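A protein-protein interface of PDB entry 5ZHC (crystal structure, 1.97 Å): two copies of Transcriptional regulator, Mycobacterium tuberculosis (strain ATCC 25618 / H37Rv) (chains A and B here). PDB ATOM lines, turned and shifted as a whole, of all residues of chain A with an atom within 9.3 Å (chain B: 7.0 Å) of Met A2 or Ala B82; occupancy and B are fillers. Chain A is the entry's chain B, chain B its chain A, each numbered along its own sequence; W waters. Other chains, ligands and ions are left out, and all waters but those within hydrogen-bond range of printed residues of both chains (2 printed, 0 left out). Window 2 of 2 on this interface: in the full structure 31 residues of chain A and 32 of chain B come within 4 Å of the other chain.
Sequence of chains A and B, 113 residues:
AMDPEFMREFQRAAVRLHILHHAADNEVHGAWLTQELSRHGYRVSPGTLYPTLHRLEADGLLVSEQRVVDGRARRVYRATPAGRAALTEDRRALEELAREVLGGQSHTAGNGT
The side-chain carboxylate (OE2) of Glu B89 is in hydrogen-bond range of the backbone NH (N) of Met A2, 2.8 Å away.
OD2 of Asp B90 sits close to OD2 of Asp A3.
O of Leu B61 lies within hydrogen-bond range of N of Thr B80 (3.1 Å).
OG1 of Thr B80 lies close to N of Ala B82.
N of Phe A6 lies within hydrogen-bond range of OD1 of Asp A3, 3.2 Å away.
Among the printed residues, pairs that only touch across the chains: Ala A1 with Glu B89 (3.8 Å), Met A2 with Leu B61 (3.6 Å), Met A2 with Ala B82 (3.2 Å), Met A2 with Ala B86 (3.7 Å), Asp A3 with Leu B20 (3.7 Å), Asp A3 with Leu B61 (3.7 Å), Asp A3 with Ala B86 (3.8 Å), Phe A6 with Asp B90 (3.2 Å), Met A7 with Glu B89 (3.6 Å) and Met A7 with Asp B90 (3.7 Å).
No residue of chain A comes within 4 Å of Pro B81.
No residue of chain A comes within 4 Å of Ala B85.
Of the printed residues of chain B, Asp A3 touches Leu B20, Leu B61, Ala B86 and Asp B90.
Printed residues of chain A within 4 Å of Ala B86: Met A2 and Asp A3.
Thr B80 touches none of the printed residues of chain A.
The nearest residue of chain B that does not touch Met A2 is Ala B85 (4.1 Å).
Printed residues of chain B that touch a printed residue of chain A: Leu B20, Leu B61, Ala B82, Ala B86, Glu B89 and Asp B90.
Among the printed residues, no Asp or Glu carboxylate lies within 4 Å of a Lys or Arg side-chain nitrogen of the other chain.
No position is printed for both chains.
Of the 12 pairs that touch across the chains among the printed residues, none has its exchanged pair printed and touching as well.
Water W2 bridges OD2 of Asp B59 (2.5 Å) and OE1 of Glu A5 (2.6 Å).
Water W1 lies within hydrogen-bond range of the backbone NH of Asp A3 (2.9 Å), the side-chain carboxylate of Glu B89 (2.9 Å), the side-chain carboxylate of Asp B90 (3.1 Å) and the backbone NH of Met A2 (3.4 Å).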
ATOM      1  N   ALA A   1      20.869  -2.352  -3.472  1.00  0.00           N
ATOM      2  CA  ALA A   1      21.726  -2.938  -2.387  1.00  0.00           C
ATOM      3  C   ALA A   1      23.177  -2.489  -2.537  1.00  0.00           C
ATOM      4  O   ALA A   1      23.755  -2.633  -3.625  1.00  0.00           O
ATOM      5  CB  ALA A   1      21.669  -4.462  -2.423  1.00  0.00           C
ATOM      6  N   MET A   2      23.786  -1.972  -1.472  1.00  0.00           N
ATOM      7  CA  MET A   2      25.209  -1.610  -1.553  1.00  0.00           C
ATOM      8  C   MET A   2      26.114  -2.865  -1.706  1.00  0.00           C
ATOM      9  O   MET A   2      27.171  -2.795  -2.354  1.00  0.00           O
ATOM     10  CB  MET A   2      25.628  -0.787  -0.343  1.00  0.00           C
ATOM     11  CG  MET A   2      25.040   0.621  -0.252  1.00  0.00           C
ATOM     12  SD  MET A   2      25.415   1.617  -1.700  1.00  0.00           S
ATOM     13  CE  MET A   2      27.182   1.676  -1.640  1.00  0.00           C
ATOM     14  N   ASP A   3      25.679  -4.009  -1.179  1.00  0.00           N
ATOM     15  CA  ASP A   3      26.471  -5.226  -1.173  1.00  0.00           C
ATOM     16  C   ASP A   3      25.661  -6.423  -1.710  1.00  0.00           C
ATOM     17  O   ASP A   3      25.238  -7.290  -0.945  1.00  0.00           O
ATOM     18  CB  ASP A   3      26.904  -5.458   0.264  1.00  0.00           C
ATOM     19  CG  ASP A   3      27.929  -6.525   0.424  1.00  0.00           C
ATOM     20  OD1 ASP A   3      28.293  -7.218  -0.540  1.00  0.00           O
ATOM     21  OD2 ASP A   3      28.350  -6.684   1.598  1.00  0.00           O
ATOM     22  N   PRO A   4      25.458  -6.473  -3.046  1.00  0.00           N
ATOM     23  CA  PRO A   4      24.637  -7.559  -3.597  1.00  0.00           C
ATOM     24  C   PRO A   4      25.209  -8.936  -3.364  1.00  0.00           C
ATOM     25  O   PRO A   4      24.435  -9.872  -3.241  1.00  0.00           O
ATOM     26  CB  PRO A   4      24.544  -7.252  -5.106  1.00  0.00           C
ATOM     27  CG  PRO A   4      25.389  -6.072  -5.352  1.00  0.00           C
ATOM     28  CD  PRO A   4      25.781  -5.449  -4.055  1.00  0.00           C
ATOM     29  N   GLU A   5      26.528  -9.085  -3.290  1.00  0.00           N
ATOM     30  CA  GLU A   5      27.091 -10.412  -3.014  1.00  0.00           C
ATOM     31  C   GLU A   5      26.731 -10.919  -1.599  1.00  0.00           C
ATOM     32  O   GLU A   5      26.353 -12.095  -1.437  1.00  0.00           O
ATOM     33  CB  GLU A   5      28.601 -10.448  -3.278  1.00  0.00           C
ATOM     34  CG  GLU A   5      29.282 -11.810  -3.035  1.00  0.00           C
ATOM     35  CD  GLU A   5      30.782 -11.917  -3.505  1.00  0.00           C
ATOM     36  OE1 GLU A   5      31.540 -10.901  -3.754  1.00  0.00           O
ATOM     37  OE2 GLU A   5      31.249 -13.081  -3.648  1.00  0.00           O
ATOM     38  N   PHE A   6      26.848 -10.047  -0.584  1.00  0.00           N
ATOM     39  CA  PHE A   6      26.376 -10.429   0.752  1.00  0.00           C
ATOM     40  C   PHE A   6      24.898 -10.831   0.659  1.00  0.00           C
ATOM     41  O   PHE A   6      24.512 -11.870   1.178  1.00  0.00           O
ATOM     42  CB  PHE A   6      26.484  -9.298   1.769  1.00  0.00           C
ATOM     43  CG  PHE A   6      25.839  -9.641   3.105  1.00  0.00           C
ATOM     44  CD1 PHE A   6      26.531 -10.347   4.076  1.00  0.00           C
ATOM     45  CD2 PHE A   6      24.519  -9.304   3.365  1.00  0.00           C
ATOM     46  CE1 PHE A   6      25.945 -10.653   5.298  1.00  0.00           C
ATOM     47  CE2 PHE A   6      23.918  -9.604   4.597  1.00  0.00           C
ATOM     48  CZ  PHE A   6      24.631 -10.279   5.558  1.00  0.00           C
ATOM     49  N   MET A   7      24.087 -10.002  -0.001  1.00  0.00           N
ATOM     50  CA  MET A   7      22.627 -10.212  -0.014  1.00  0.00           C
ATOM     51  C   MET A   7      22.261 -11.518  -0.693  1.00  0.00           C
ATOM     52  O   MET A   7      21.377 -12.237  -0.241  1.00  0.00           O
ATOM     53  CB  MET A   7      21.863  -9.016  -0.605  1.00  0.00           C
ATOM     54  CG  MET A   7      21.939  -7.750   0.243  1.00  0.00           C
ATOM     55  SD  MET A   7      21.173  -7.857   1.879  1.00  0.00           S
ATOM     56  CE  MET A   7      21.581  -6.190   2.367  1.00  0.00           C
ATOM     57  N   LEU B  20      33.911  -6.281   6.675  1.00  0.00           N
ATOM     58  CA  LEU B  20      33.462  -4.880   6.664  1.00  0.00           C
ATOM     59  C   LEU B  20      33.462  -4.296   8.064  1.00  0.00           C
ATOM     60  O   LEU B  20      33.888  -3.158   8.255  1.00  0.00           O
ATOM     61  CB  LEU B  20      32.065  -4.743   6.051  1.00  0.00           C
ATOM     62  CG  LEU B  20      31.960  -5.049   4.564  1.00  0.00           C
ATOM     63  CD1 LEU B  20      30.517  -4.997   4.132  1.00  0.00           C
ATOM     64  CD2 LEU B  20      32.803  -4.082   3.725  1.00  0.00           C
ATOM     65  N   ASP B  59      33.859  -3.888  -5.769  1.00  0.00           N
ATOM     66  CA  ASP B  59      32.520  -3.418  -5.474  1.00  0.00           C
ATOM     67  C   ASP B  59      32.504  -2.002  -4.882  1.00  0.00           C
ATOM     68  O   ASP B  59      31.436  -1.451  -4.645  1.00  0.00           O
ATOM     69  CB  ASP B  59      31.796  -4.380  -4.514  1.00  0.00           C
ATOM     70  CG  ASP B  59      31.470  -5.750  -5.131  1.00  0.00           C
ATOM     71  OD1 ASP B  59      31.555  -5.926  -6.366  1.00  0.00           O
ATOM     72  OD2 ASP B  59      31.173  -6.703  -4.373  1.00  0.00           O
ATOM     73  N   GLY B  60      33.655  -1.437  -4.569  1.00  0.00           N
ATOM     74  CA  GLY B  60      33.733  -0.083  -4.022  1.00  0.00           C
ATOM     75  C   GLY B  60      33.496  -0.001  -2.521  1.00  0.00           C
ATOM     76  O   GLY B  60      33.332   1.085  -1.974  1.00  0.00           O
ATOM     77  N   LEU B  61      33.540  -1.147  -1.852  1.00  0.00           N
ATOM     78  CA  LEU B  61      33.204  -1.250  -0.426  1.00  0.00           C
ATOM     79  C   LEU B  61      34.452  -1.185   0.456  1.00  0.00           C
ATOM     80  O   LEU B  61      34.395  -0.754   1.614  1.00  0.00           O
ATOM     81  CB  LEU B  61      32.415  -2.534  -0.144  1.00  0.00           C
ATOM     82  CG  LEU B  61      31.135  -2.699  -0.990  1.00  0.00           C
ATOM     83  CD1 LEU B  61      30.363  -3.933  -0.583  1.00  0.00           C
ATOM     84  CD2 LEU B  61      30.240  -1.495  -0.913  1.00  0.00           C
ATOM     85  N   LEU B  62      35.569  -1.618  -0.095  1.00  0.00           N
ATOM     86  CA  LEU B  62      36.884  -1.416   0.498  1.00  0.00           C
ATOM     87  C   LEU B  62      37.748  -0.616  -0.458  1.00  0.00           C
ATOM     88  O   LEU B  62      37.518  -0.629  -1.652  1.00  0.00           O
ATOM     89  CB  LEU B  62      37.591  -2.743   0.752  1.00  0.00           C
ATOM     90  CG  LEU B  62      36.998  -3.727   1.759  1.00  0.00           C
ATOM     91  CD1 LEU B  62      37.901  -4.965   1.830  1.00  0.00           C
ATOM     92  CD2 LEU B  62      36.792  -3.135   3.126  1.00  0.00           C
ATOM     93  N   ALA B  79      37.410   0.379   4.979  1.00  0.00           N
ATOM     94  CA  ALA B  79      36.087   0.523   4.421  1.00  0.00           C
ATOM     95  C   ALA B  79      35.984   1.914   3.812  1.00  0.00           C
ATOM     96  O   ALA B  79      36.557   2.865   4.314  1.00  0.00           O
ATOM     97  CB  ALA B  79      35.009   0.371   5.475  1.00  0.00           C
ATOM     98  N   THR B  80      35.261   1.988   2.710  1.00  0.00           N
ATOM     99  CA  THR B  80      34.911   3.251   2.109  1.00  0.00           C
ATOM    100  C   THR B  80      33.600   3.712   2.723  1.00  0.00           C
ATOM    101  O   THR B  80      32.924   2.945   3.412  1.00  0.00           O
ATOM    102  CB  THR B  80      34.668   3.076   0.591  1.00  0.00           C
ATOM    103  OG1 THR B  80      33.614   2.144   0.384  1.00  0.00           O
ATOM    104  CG2 THR B  80      35.989   2.585  -0.131  1.00  0.00           C
ATOM    105  N   PRO B  81      33.194   4.960   2.434  1.00  0.00           N
ATOM    106  CA  PRO B  81      31.828   5.346   2.800  1.00  0.00           C
ATOM    107  C   PRO B  81      30.736   4.383   2.247  1.00  0.00           C
ATOM    108  O   PRO B  81      29.797   4.043   2.971  1.00  0.00           O
ATOM    109  CB  PRO B  81      31.727   6.783   2.264  1.00  0.00           C
ATOM    110  CG  PRO B  81      33.141   7.289   2.231  1.00  0.00           C
ATOM    111  CD  PRO B  81      33.968   6.090   1.864  1.00  0.00           C
ATOM    112  N   ALA B  82      30.878   3.888   1.012  1.00  0.00           N
ATOM    113  CA  ALA B  82      29.925   2.887   0.487  1.00  0.00           C
ATOM    114  C   ALA B  82      29.963   1.592   1.336  1.00  0.00           C
ATOM    115  O   ALA B  82      28.942   0.965   1.571  1.00  0.00           O
ATOM    116  CB  ALA B  82      30.210   2.569  -0.981  1.00  0.00           C
ATOM    117  N   GLY B  83      31.148   1.189   1.757  1.00  0.00           N
ATOM    118  CA  GLY B  83      31.323   0.026   2.646  1.00  0.00           C
ATOM    119  C   GLY B  83      30.653   0.178   4.016  1.00  0.00           C
ATOM    120  O   GLY B  83      30.073  -0.774   4.554  1.00  0.00           O
ATOM    121  N   ARG B  84      30.737   1.379   4.588  1.00  0.00           N
ATOM    122  CA  ARG B  84      30.037   1.623   5.832  1.00  0.00           C
ATOM    123  C   ARG B  84      28.540   1.520   5.640  1.00  0.00           C
ATOM    124  O   ARG B  84      27.861   0.888   6.432  1.00  0.00           O
ATOM    125  CB  ARG B  84      30.399   2.974   6.427  1.00  0.00           C
ATOM    126  CG  ARG B  84      31.859   3.053   6.807  1.00  0.00           C
ATOM    127  CD  ARG B  84      32.294   4.491   7.134  1.00  0.00           C
ATOM    128  NE  ARG B  84      33.740   4.452   7.330  1.00  0.00           N
ATOM    129  CZ  ARG B  84      34.337   3.968   8.417  1.00  0.00           C
ATOM    130  NH1 ARG B  84      33.612   3.548   9.459  1.00  0.00           N
ATOM    131  NH2 ARG B  84      35.663   3.904   8.468  1.00  0.00           N
ATOM    132  N   ALA B  85      28.026   2.096   4.558  1.00  0.00           N
ATOM    133  CA  ALA B  85      26.591   1.980   4.232  1.00  0.00           C
ATOM    134  C   ALA B  85      26.203   0.492   4.012  1.00  0.00           C
ATOM    135  O   ALA B  85      25.179   0.046   4.501  1.00  0.00           O
ATOM    136  CB  ALA B  85      26.223   2.851   3.017  1.00  0.00           C
ATOM    137  N   ALA B  86      27.042  -0.260   3.298  1.00  0.00           N
ATOM    138  CA  ALA B  86      26.811  -1.691   3.105  1.00  0.00           C
ATOM    139  C   ALA B  86      26.769  -2.481   4.420  1.00  0.00           C
ATOM    140  O   ALA B  86      25.953  -3.384   4.594  1.00  0.00           O
ATOM    141  CB  ALA B  86      27.869  -2.306   2.214  1.00  0.00           C
ATOM    142  N   LEU B  87      27.707  -2.157   5.300  1.00  0.00           N
ATOM    143  CA  LEU B  87      27.737  -2.756   6.636  1.00  0.00           C
ATOM    144  C   LEU B  87      26.393  -2.564   7.352  1.00  0.00           C
ATOM    145  O   LEU B  87      25.825  -3.503   7.898  1.00  0.00           O
ATOM    146  CB  LEU B  87      28.904  -2.171   7.432  1.00  0.00           C
ATOM    147  CG  LEU B  87      29.122  -2.656   8.865  1.00  0.00           C
ATOM    148  CD1 LEU B  87      29.234  -4.174   8.990  1.00  0.00           C
ATOM    149  CD2 LEU B  87      30.346  -1.938   9.408  1.00  0.00           C
ATOM    150  N   THR B  88      25.849  -1.347   7.279  1.00  0.00           N
ATOM    151  CA  THR B  88      24.529  -1.072   7.872  1.00  0.00           C
ATOM    152  C   THR B  88      23.419  -1.910   7.241  1.00  0.00           C
ATOM    153  O   THR B  88      22.603  -2.490   7.941  1.00  0.00           O
ATOM    154  CB  THR B  88      24.182   0.418   7.743  1.00  0.00           C
ATOM    155  OG1 THR B  88      25.134   1.134   8.516  1.00  0.00           O
ATOM    156  CG2 THR B  88      22.762   0.735   8.266  1.00  0.00           C
ATOM    157  N   GLU B  89      23.421  -2.025   5.914  1.00  0.00           N
ATOM    158  CA  GLU B  89      22.380  -2.798   5.218  1.00  0.00           C
ATOM    159  C   GLU B  89      22.511  -4.303   5.524  1.00  0.00           C
ATOM    160  O   GLU B  89      21.512  -5.006   5.723  1.00  0.00           O
ATOM    161  CB  GLU B  89      22.397  -2.531   3.711  1.00  0.00           C
ATOM    162  CG  GLU B  89      22.095  -1.078   3.345  1.00  0.00           C
ATOM    163  CD  GLU B  89      22.364  -0.726   1.876  1.00  0.00           C
ATOM    164  OE1 GLU B  89      22.195   0.481   1.514  1.00  0.00           O
ATOM    165  OE2 GLU B  89      22.790  -1.632   1.095  1.00  0.00           O
ATOM    166  N   ASP B  90      23.758  -4.784   5.548  1.00  0.00           N
ATOM    167  CA  ASP B  90      24.020  -6.197   5.828  1.00  0.00           C
ATOM    168  C   ASP B  90      23.570  -6.535   7.265  1.00  0.00           C
ATOM    169  O   ASP B  90      22.954  -7.564   7.500  1.00  0.00           O
ATOM    170  CB  ASP B  90      25.495  -6.559   5.626  1.00  0.00           C
ATOM    171  CG  ASP B  90      25.983  -6.384   4.148  1.00  0.00           C
ATOM    172  OD1 ASP B  90      25.189  -6.144   3.209  1.00  0.00           O
ATOM    173  OD2 ASP B  90      27.212  -6.474   3.922  1.00  0.00           O
HETATM  174  O   HOH W   1      23.983  -4.249   1.103  1.00  0.00           O
HETATM  175  O   HOH W   2      31.068  -8.926  -5.414  1.00  0.00           O
